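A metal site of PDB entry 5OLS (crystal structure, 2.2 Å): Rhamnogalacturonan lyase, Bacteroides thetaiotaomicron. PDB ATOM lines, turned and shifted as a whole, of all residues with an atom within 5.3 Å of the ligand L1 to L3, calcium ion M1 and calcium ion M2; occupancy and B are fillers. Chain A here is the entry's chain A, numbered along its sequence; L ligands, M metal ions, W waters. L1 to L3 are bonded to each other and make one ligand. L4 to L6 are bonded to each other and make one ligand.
Within 4 Å of calcium ion M1: Gly 191, Asp 225 and Asp 259. The nearest printed residue that does not touch calcium ion M1 is Asn 192 (4.7 Å).
Calcium ion M2 is bound by OD2 of Asp 225, at 2.2 Å. Water W3 binds calcium ion M2 (2.3 Å). OD1 of Asp 194 is bound to calcium ion M2 (2.3 Å). O2 of LG3 L3 binds calcium ion M2. OD2 of Asp 194 is bound to calcium ion M2 (2.5 Å). Calcium ion M2 is bound by OD2 of Asp 229 (2.5 Å). OD2 of Asp 226 is bound to calcium ion M2, 2.5 Å away.
Water W1 bridges OD1 of Asp 226 (3.4 Å) and O2 of LG2 L2 (3.5 Å).
SD of Met 270 lies close to ND1 of His 304, 3.8 Å away. The backbone carbonyl oxygen (O) of Ile 231 is in hydrogen-bond range of a ring nitrogen (ND1) of His 199, at 2.5 Å. OH of Tyr 301 is in hydrogen-bond range of NE2 of His 304 (2.9 Å). The backbone NH (N) of Ile 231 is in hydrogen-bond range of the side-chain carboxylate (OD1) of Asp 229.
A ring nitrogen (NE2) of His 304 is in hydrogen-bond range of an oxygen (O7) of LIG L1 (3.0 Å). The side-chain hydroxyl (OH) of Tyr 301 is in hydrogen-bond range of an oxygen (O6) of LIG L1 (3.0 Å). The guanidinium group of Arg 298 lies within salt-bridge range of an oxygen (O6) of LIG L1 (3.2 Å). O2 of LG2 L2 is in hydrogen-bond range of OD1 of Asn 303 (3.0 Å).
Calcium ion M1 is bound by O3 of LG3 L3 (2.4 Å), water W2 (2.4 Å), O of Gly 191 (2.4 Å), OD2 of Asp 225 (2.8 Å), OD1 of Asp 225 (2.8 Å), OD2 of Asp 259 (2.8 Å) and O2 of LG3 L3 (2.9 Å).
Merely in contact with the ligand L1 to L3: Ile 231, Met 270 and Leu 297. Hydrophobic or aromatic side chains that line the ligand L1 to L3: Ile 231, Met 270, Leu 297, Tyr 301 and His 304. 11 residues have an atom within 4 Å of the ligand L1 to L3: Asp 225, Asp 226, Asp 229, Ile 231, Asp 259, Met 270, Leu 297, Arg 298, Tyr 301, Asn 303 and His 304.
An oxygen (O4) of LG3 L3 is in hydrogen-bond range of an oxygen (O1) of LG4 L4, 2.7 Å away.
Of the 19 residues printed, 4 come within 4 Å of calcium ion M2. The nearest printed residue that does not touch calcium ion M2 is Gly 191 (4.8 Å).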
ATOM      1  N   LYS A 189      16.702 -33.051 -11.600  1.00  0.00           N
ATOM      2  CA  LYS A 189      17.566 -31.983 -12.142  1.00  0.00           C
ATOM      3  C   LYS A 189      17.404 -30.682 -11.345  1.00  0.00           C
ATOM      4  O   LYS A 189      18.384 -29.996 -11.065  1.00  0.00           O
ATOM      5  CB  LYS A 189      17.261 -31.722 -13.637  1.00  0.00           C
ATOM      6  CG  LYS A 189      18.156 -30.683 -14.328  1.00  0.00           C
ATOM      7  CD  LYS A 189      19.540 -31.237 -14.648  1.00  0.00           C
ATOM      8  CE  LYS A 189      20.591 -30.138 -14.882  1.00  0.00           C
ATOM      9  NZ  LYS A 189      20.784 -29.738 -16.299  1.00  0.00           N
ATOM     10  N   GLY A 191      15.920 -28.064 -12.544  1.00  0.00           N
ATOM     11  CA  GLY A 191      16.189 -27.021 -13.528  1.00  0.00           C
ATOM     12  C   GLY A 191      15.142 -25.915 -13.667  1.00  0.00           C
ATOM     13  O   GLY A 191      15.327 -24.989 -14.471  1.00  0.00           O
ATOM     14  N   ASN A 192      14.048 -26.015 -12.922  1.00  0.00           N
ATOM     15  CA  ASN A 192      12.942 -25.055 -12.985  1.00  0.00           C
ATOM     16  C   ASN A 192      12.747 -24.249 -11.694  1.00  0.00           C
ATOM     17  O   ASN A 192      11.905 -23.337 -11.658  1.00  0.00           O
ATOM     18  CB  ASN A 192      11.656 -25.804 -13.338  1.00  0.00           C
ATOM     19  CG  ASN A 192      11.659 -26.349 -14.761  1.00  0.00           C
ATOM     20  OD1 ASN A 192      12.443 -25.944 -15.600  1.00  0.00           O
ATOM     21  ND2 ASN A 192      10.744 -27.274 -15.037  1.00  0.00           N
ATOM     22  N   ASP A 194      13.833 -21.603  -9.407  1.00  0.00           N
ATOM     23  CA  ASP A 194      14.506 -20.351  -9.094  1.00  0.00           C
ATOM     24  C   ASP A 194      14.038 -19.745  -7.777  1.00  0.00           C
ATOM     25  O   ASP A 194      12.927 -20.035  -7.279  1.00  0.00           O
ATOM     26  CB  ASP A 194      14.258 -19.295 -10.194  1.00  0.00           C
ATOM     27  CG  ASP A 194      14.880 -19.658 -11.545  1.00  0.00           C
ATOM     28  OD1 ASP A 194      15.810 -20.496 -11.626  1.00  0.00           O
ATOM     29  OD2 ASP A 194      14.436 -19.085 -12.571  1.00  0.00           O
ATOM     30  N   HIS A 199       9.201 -12.866 -15.380  1.00  0.00           N
ATOM     31  CA  HIS A 199       8.898 -13.417 -16.715  1.00  0.00           C
ATOM     32  C   HIS A 199       7.588 -12.835 -17.265  1.00  0.00           C
ATOM     33  O   HIS A 199       6.661 -13.569 -17.659  1.00  0.00           O
ATOM     34  CB  HIS A 199       8.830 -14.941 -16.663  1.00  0.00           C
ATOM     35  CG  HIS A 199       9.961 -15.562 -15.902  1.00  0.00           C
ATOM     36  ND1 HIS A 199      11.263 -15.458 -16.309  1.00  0.00           N
ATOM     37  CD2 HIS A 199       9.968 -16.255 -14.749  1.00  0.00           C
ATOM     38  CE1 HIS A 199      12.038 -16.080 -15.444  1.00  0.00           C
ATOM     39  NE2 HIS A 199      11.278 -16.577 -14.484  1.00  0.00           N
ATOM     40  N   ASP A 225      18.148 -24.223  -9.413  1.00  0.00           N
ATOM     41  CA  ASP A 225      18.461 -23.609 -10.709  1.00  0.00           C
ATOM     42  C   ASP A 225      19.208 -22.253 -10.549  1.00  0.00           C
ATOM     43  O   ASP A 225      20.449 -22.226 -10.401  1.00  0.00           O
ATOM     44  CB  ASP A 225      17.214 -23.524 -11.592  1.00  0.00           C
ATOM     45  CG  ASP A 225      17.532 -23.230 -13.055  1.00  0.00           C
ATOM     46  OD1 ASP A 225      18.377 -23.952 -13.643  1.00  0.00           O
ATOM     47  OD2 ASP A 225      16.888 -22.303 -13.644  1.00  0.00           O
ATOM     48  N   ASP A 226      18.479 -21.139 -10.553  1.00  0.00           N
ATOM     49  CA  ASP A 226      19.083 -19.825 -10.430  1.00  0.00           C
ATOM     50  C   ASP A 226      18.583 -19.156  -9.170  1.00  0.00           C
ATOM     51  O   ASP A 226      17.585 -19.585  -8.556  1.00  0.00           O
ATOM     52  CB  ASP A 226      18.754 -18.983 -11.653  1.00  0.00           C
ATOM     53  CG  ASP A 226      19.212 -19.634 -12.947  1.00  0.00           C
ATOM     54  OD1 ASP A 226      20.329 -20.197 -13.014  1.00  0.00           O
ATOM     55  OD2 ASP A 226      18.470 -19.546 -13.929  1.00  0.00           O
ATOM     56  N   ASP A 229      16.200 -14.703 -12.118  1.00  0.00           N
ATOM     57  CA  ASP A 229      16.077 -15.044 -13.536  1.00  0.00           C
ATOM     58  C   ASP A 229      15.019 -14.146 -14.188  1.00  0.00           C
ATOM     59  O   ASP A 229      13.862 -14.122 -13.736  1.00  0.00           O
ATOM     60  CB  ASP A 229      15.692 -16.523 -13.638  1.00  0.00           C
ATOM     61  CG  ASP A 229      15.565 -17.034 -15.072  1.00  0.00           C
ATOM     62  OD1 ASP A 229      15.600 -16.228 -16.028  1.00  0.00           O
ATOM     63  OD2 ASP A 229      15.412 -18.281 -15.216  1.00  0.00           O
ATOM     64  N   ILE A 231      14.385 -14.247 -17.749  1.00  0.00           N
ATOM     65  CA  ILE A 231      14.193 -14.730 -19.100  1.00  0.00           C
ATOM     66  C   ILE A 231      12.735 -14.518 -19.467  1.00  0.00           C
ATOM     67  O   ILE A 231      11.870 -14.535 -18.592  1.00  0.00           O
ATOM     68  CB  ILE A 231      14.606 -16.220 -19.253  1.00  0.00           C
ATOM     69  CG1 ILE A 231      15.044 -16.496 -20.698  1.00  0.00           C
ATOM     70  CG2 ILE A 231      13.479 -17.164 -18.806  1.00  0.00           C
ATOM     71  CD1 ILE A 231      15.410 -17.943 -20.984  1.00  0.00           C
ATOM     72  N   ASP A 259      21.155 -24.563 -13.540  1.00  0.00           N
ATOM     73  CA  ASP A 259      22.064 -23.682 -14.297  1.00  0.00           C
ATOM     74  C   ASP A 259      23.036 -22.868 -13.476  1.00  0.00           C
ATOM     75  O   ASP A 259      24.049 -22.393 -14.001  1.00  0.00           O
ATOM     76  CB  ASP A 259      21.264 -22.733 -15.191  1.00  0.00           C
ATOM     77  CG  ASP A 259      20.356 -23.474 -16.147  1.00  0.00           C
ATOM     78  OD1 ASP A 259      20.590 -24.662 -16.379  1.00  0.00           O
ATOM     79  OD2 ASP A 259      19.390 -22.880 -16.639  1.00  0.00           O
ATOM     80  N   GLY A 267      17.247 -12.462 -21.658  1.00  0.00           N
ATOM     81  CA  GLY A 267      17.227 -13.617 -22.531  1.00  0.00           C
ATOM     82  C   GLY A 267      15.842 -13.981 -23.003  1.00  0.00           C
ATOM     83  O   GLY A 267      14.852 -13.738 -22.308  1.00  0.00           O
ATOM     84  N   GLY A 269      15.852 -17.196 -24.792  1.00  0.00           N
ATOM     85  CA  GLY A 269      16.214 -18.537 -25.204  1.00  0.00           C
ATOM     86  C   GLY A 269      17.015 -18.572 -26.492  1.00  0.00           C
ATOM     87  O   GLY A 269      17.012 -17.629 -27.290  1.00  0.00           O
ATOM     88  N   MET A 270      17.674 -19.701 -26.681  1.00  0.00           N
ATOM     89  CA  MET A 270      18.415 -19.994 -27.891  1.00  0.00           C
ATOM     90  C   MET A 270      17.806 -21.260 -28.503  1.00  0.00           C
ATOM     91  O   MET A 270      18.512 -22.216 -28.799  1.00  0.00           O
ATOM     92  CB  MET A 270      19.891 -20.202 -27.556  1.00  0.00           C
ATOM     93  CG  MET A 270      20.559 -18.982 -26.947  1.00  0.00           C
ATOM     94  SD  MET A 270      20.898 -17.737 -28.193  1.00  0.00           S
ATOM     95  CE  MET A 270      22.410 -18.396 -28.880  1.00  0.00           C
ATOM     96  N   ARG A 296      26.928 -21.915  -9.042  1.00  0.00           N
ATOM     97  CA  ARG A 296      27.612 -23.014  -9.707  1.00  0.00           C
ATOM     98  C   ARG A 296      28.428 -22.544 -10.916  1.00  0.00           C
ATOM     99  O   ARG A 296      29.584 -22.948 -11.064  1.00  0.00           O
ATOM    100  CB  ARG A 296      26.665 -24.146 -10.128  1.00  0.00           C
ATOM    101  CG  ARG A 296      27.380 -25.431 -10.506  1.00  0.00           C
ATOM    102  CD  ARG A 296      26.427 -26.617 -10.652  1.00  0.00           C
ATOM    103  NE  ARG A 296      25.641 -26.572 -11.887  1.00  0.00           N
ATOM    104  CZ  ARG A 296      26.111 -26.846 -13.110  1.00  0.00           C
ATOM    105  NH1 ARG A 296      25.295 -26.758 -14.155  1.00  0.00           N
ATOM    106  NH2 ARG A 296      27.385 -27.200 -13.304  1.00  0.00           N
ATOM    107  N   LEU A 297      27.849 -21.688 -11.754  1.00  0.00           N
ATOM    108  CA  LEU A 297      28.436 -21.380 -13.066  1.00  0.00           C
ATOM    109  C   LEU A 297      28.682 -19.907 -13.328  1.00  0.00           C
ATOM    110  O   LEU A 297      29.743 -19.553 -13.837  1.00  0.00           O
ATOM    111  CB  LEU A 297      27.572 -21.958 -14.200  1.00  0.00           C
ATOM    112  CG  LEU A 297      27.719 -23.462 -14.460  1.00  0.00           C
ATOM    113  CD1 LEU A 297      26.740 -23.957 -15.526  1.00  0.00           C
ATOM    114  CD2 LEU A 297      29.152 -23.822 -14.865  1.00  0.00           C
ATOM    115  N   ARG A 298      27.714 -19.052 -13.026  1.00  0.00           N
ATOM    116  CA  ARG A 298      27.812 -17.645 -13.391  1.00  0.00           C
ATOM    117  C   ARG A 298      27.177 -16.721 -12.323  1.00  0.00           C
ATOM    118  O   ARG A 298      26.288 -17.128 -11.559  1.00  0.00           O
ATOM    119  CB  ARG A 298      27.183 -17.394 -14.766  1.00  0.00           C
ATOM    120  CG  ARG A 298      27.493 -18.402 -15.883  1.00  0.00           C
ATOM    121  CD  ARG A 298      26.702 -18.044 -17.143  1.00  0.00           C
ATOM    122  NE  ARG A 298      27.073 -18.777 -18.351  1.00  0.00           N
ATOM    123  CZ  ARG A 298      26.609 -19.980 -18.716  1.00  0.00           C
ATOM    124  NH1 ARG A 298      25.774 -20.680 -17.951  1.00  0.00           N
ATOM    125  NH2 ARG A 298      27.008 -20.512 -19.860  1.00  0.00           N
ATOM    126  N   TYR A 301      24.777 -12.162 -15.442  1.00  0.00           N
ATOM    127  CA  TYR A 301      24.704 -12.798 -16.761  1.00  0.00           C
ATOM    128  C   TYR A 301      23.577 -12.228 -17.625  1.00  0.00           C
ATOM    129  O   TYR A 301      22.430 -12.160 -17.197  1.00  0.00           O
ATOM    130  CB  TYR A 301      24.485 -14.295 -16.545  1.00  0.00           C
ATOM    131  CG  TYR A 301      24.482 -15.204 -17.767  1.00  0.00           C
ATOM    132  CD1 TYR A 301      25.298 -14.982 -18.874  1.00  0.00           C
ATOM    133  CD2 TYR A 301      23.677 -16.351 -17.778  1.00  0.00           C
ATOM    134  CE1 TYR A 301      25.302 -15.850 -19.976  1.00  0.00           C
ATOM    135  CE2 TYR A 301      23.681 -17.228 -18.862  1.00  0.00           C
ATOM    136  CZ  TYR A 301      24.489 -16.975 -19.965  1.00  0.00           C
ATOM    137  OH  TYR A 301      24.474 -17.855 -21.038  1.00  0.00           O
ATOM    138  N   ASN A 303      22.559 -13.512 -20.454  1.00  0.00           N
ATOM    139  CA  ASN A 303      21.721 -14.671 -20.692  1.00  0.00           C
ATOM    140  C   ASN A 303      21.096 -14.617 -22.097  1.00  0.00           C
ATOM    141  O   ASN A 303      19.922 -14.860 -22.241  1.00  0.00           O
ATOM    142  CB  ASN A 303      20.636 -14.762 -19.598  1.00  0.00           C
ATOM    143  CG  ASN A 303      19.993 -16.135 -19.504  1.00  0.00           C
ATOM    144  OD1 ASN A 303      20.681 -17.147 -19.548  1.00  0.00           O
ATOM    145  ND2 ASN A 303      18.668 -16.166 -19.360  1.00  0.00           N
ATOM    146  N   HIS A 304      21.911 -14.283 -23.094  1.00  0.00           N
ATOM    147  CA  HIS A 304      21.466 -14.237 -24.499  1.00  0.00           C
ATOM    148  C   HIS A 304      20.371 -13.181 -24.761  1.00  0.00           C
ATOM    149  O   HIS A 304      19.453 -13.401 -25.551  1.00  0.00           O
ATOM    150  CB  HIS A 304      21.032 -15.644 -24.975  1.00  0.00           C
ATOM    151  CG  HIS A 304      21.917 -16.751 -24.496  1.00  0.00           C
ATOM    152  ND1 HIS A 304      23.065 -17.126 -25.163  1.00  0.00           N
ATOM    153  CD2 HIS A 304      21.840 -17.537 -23.395  1.00  0.00           C
ATOM    154  CE1 HIS A 304      23.652 -18.109 -24.498  1.00  0.00           C
ATOM    155  NE2 HIS A 304      22.923 -18.377 -23.417  1.00  0.00           N
HETATM  156  C1  LIG L   1      24.545 -24.597 -19.437  1.00  0.00           C
HETATM  157  C2  LIG L   1      23.136 -25.103 -19.176  1.00  0.00           C
HETATM  158  C3  LIG L   1      22.384 -25.077 -20.511  1.00  0.00           C
HETATM  159  C4  LIG L   1      22.352 -23.657 -21.076  1.00  0.00           C
HETATM  160  C5  LIG L   1      23.768 -23.013 -21.069  1.00  0.00           C
HETATM  161  C6  LIG L   1      23.728 -21.540 -21.419  1.00  0.00           C
HETATM  162  O1  LIG L   1      25.325 -24.781 -18.259  1.00  0.00           O
HETATM  163  O2  LIG L   1      23.123 -26.397 -18.570  1.00  0.00           O
HETATM  164  O3  LIG L   1      21.044 -25.568 -20.290  1.00  0.00           O
HETATM  165  O4  LIG L   1      21.380 -22.983 -20.216  1.00  0.00           O
HETATM  166  O5  LIG L   1      24.433 -23.203 -19.800  1.00  0.00           O
HETATM  167  O6  LIG L   1      23.745 -20.715 -20.484  1.00  0.00           O
HETATM  168  O7  LIG L   1      23.692 -21.169 -22.617  1.00  0.00           O
HETATM  169  C1  LG2 L   2      20.508 -21.962 -20.794  1.00  0.00           C
HETATM  170  C2  LG2 L   2      19.385 -21.433 -19.897  1.00  0.00           C
HETATM  171  C3  LG2 L   2      19.374 -19.953 -20.289  1.00  0.00           C
HETATM  172  C4  LG2 L   2      19.007 -19.811 -21.762  1.00  0.00           C
HETATM  173  C5  LG2 L   2      19.996 -20.610 -22.640  1.00  0.00           C
HETATM  174  C6  LG2 L   2      19.616 -20.629 -24.101  1.00  0.00           C
HETATM  175  O1  LG2 L   2      18.123 -22.119 -20.198  1.00  0.00           O
HETATM  176  O2  LG2 L   2      18.502 -19.210 -19.444  1.00  0.00           O
HETATM  177  O3  LG2 L   2      18.966 -18.414 -22.115  1.00  0.00           O
HETATM  178  O4  LG2 L   2      20.133 -21.963 -22.180  1.00  0.00           O
HETATM  179  O1  LG3 L   3      14.936 -19.774 -17.369  1.00  0.00           O
HETATM  180  C1  LG3 L   3      15.793 -20.778 -17.261  1.00  0.00           C
HETATM  181  O2  LG3 L   3      16.408 -20.920 -16.200  1.00  0.00           O
HETATM  182  C2  LG3 L   3      15.973 -21.634 -18.265  1.00  0.00           C
HETATM  183  O3  LG3 L   3      16.942 -22.706 -18.094  1.00  0.00           O
HETATM  184  C3  LG3 L   3      15.281 -21.550 -19.429  1.00  0.00           C
HETATM  185  C4  LG3 L   3      15.373 -22.642 -20.488  1.00  0.00           C
HETATM  186  O4  LG3 L   3      14.067 -23.196 -20.711  1.00  0.00           O
HETATM  187  C5  LG3 L   3      16.333 -23.761 -20.084  1.00  0.00           C
HETATM  188  O5  LG3 L   3      16.726 -24.471 -21.270  1.00  0.00           O
HETATM  189  C6  LG3 L   3      17.518 -23.157 -19.330  1.00  0.00           C
HETATM  190  C1  LG4 L   4      11.494 -21.851 -18.953  1.00  0.00           C
HETATM  191  C2  LG4 L   4      10.204 -22.665 -18.803  1.00  0.00           C
HETATM  192  C3  LG4 L   4       9.986 -22.956 -17.332  1.00  0.00           C
HETATM  193  C4  LG4 L   4      10.078 -21.700 -16.469  1.00  0.00           C
HETATM  194  C5  LG4 L   4      11.321 -20.868 -16.764  1.00  0.00           C
HETATM  195  C6  LG4 L   4      11.275 -19.513 -16.069  1.00  0.00           C
HETATM  196  O1  LG4 L   4      12.602 -22.650 -18.533  1.00  0.00           O
HETATM  197  O2  LG4 L   4       9.101 -21.893 -19.303  1.00  0.00           O
HETATM  198  O3  LG4 L   4       8.712 -23.569 -17.141  1.00  0.00           O
HETATM  199  O4  LG4 L   4      10.093 -22.099 -15.095  1.00  0.00           O
HETATM  200  O5  LG4 L   4      11.420 -20.646 -18.174  1.00  0.00           O
HETATM  201  C1  LG5 L   5       8.282 -22.516 -20.327  1.00  0.00           C
HETATM  202  C2  LG5 L   5       7.630 -21.404 -21.137  1.00  0.00           C
HETATM  203  C3  LG5 L   5       6.629 -20.623 -20.290  1.00  0.00           C
HETATM  204  C4  LG5 L   5       5.605 -21.530 -19.629  1.00  0.00           C
HETATM  205  C5  LG5 L   5       6.361 -22.672 -18.928  1.00  0.00           C
HETATM  206  C6  LG5 L   5       5.509 -23.667 -18.195  1.00  0.00           C
HETATM  207  O1  LG5 L   5       8.644 -20.517 -21.618  1.00  0.00           O
HETATM  208  O2  LG5 L   5       5.971 -19.676 -21.147  1.00  0.00           O
HETATM  209  O3  LG5 L   5       4.758 -21.969 -20.685  1.00  0.00           O
HETATM  210  O4  LG5 L   5       7.219 -23.353 -19.853  1.00  0.00           O
HETATM  211  O5  LG5 L   5       5.514 -24.853 -18.594  1.00  0.00           O
HETATM  212  O6  LG5 L   5       4.869 -23.289 -17.192  1.00  0.00           O
HETATM  213  C1  LG6 L   6       3.383 -21.660 -20.664  1.00  0.00           C
HETATM  214  C2  LG6 L   6       2.796 -21.374 -22.002  1.00  0.00           C
HETATM  215  C3  LG6 L   6       2.485 -22.709 -22.638  1.00  0.00           C
HETATM  216  C4  LG6 L   6       1.698 -23.594 -21.676  1.00  0.00           C
HETATM  217  C5  LG6 L   6       2.130 -23.513 -20.187  1.00  0.00           C
HETATM  218  C6  LG6 L   6       1.023 -24.090 -19.306  1.00  0.00           C
HETATM  219  O1  LG6 L   6       1.598 -20.580 -21.852  1.00  0.00           O
HETATM  220  O2  LG6 L   6       1.774 -22.454 -23.852  1.00  0.00           O
HETATM  221  O3  LG6 L   6       1.887 -24.945 -22.120  1.00  0.00           O
HETATM  222  O4  LG6 L   6       2.502 -22.187 -19.724  1.00  0.00           O
HETATM  223 CA    CA M   1      16.784 -23.761 -15.974  1.00  0.00          CA
HETATM  224 CA    CA M   2      16.081 -20.292 -13.932  1.00  0.00          CA
HETATM  225  O   HOH W   1      19.162 -20.361 -16.237  1.00  0.00           O
HETATM  226  O   HOH W   2      16.884 -25.922 -17.031  1.00  0.00           O
HETATM  227  O   HOH W   3      14.205 -21.563 -14.457  1.00  0.00           O
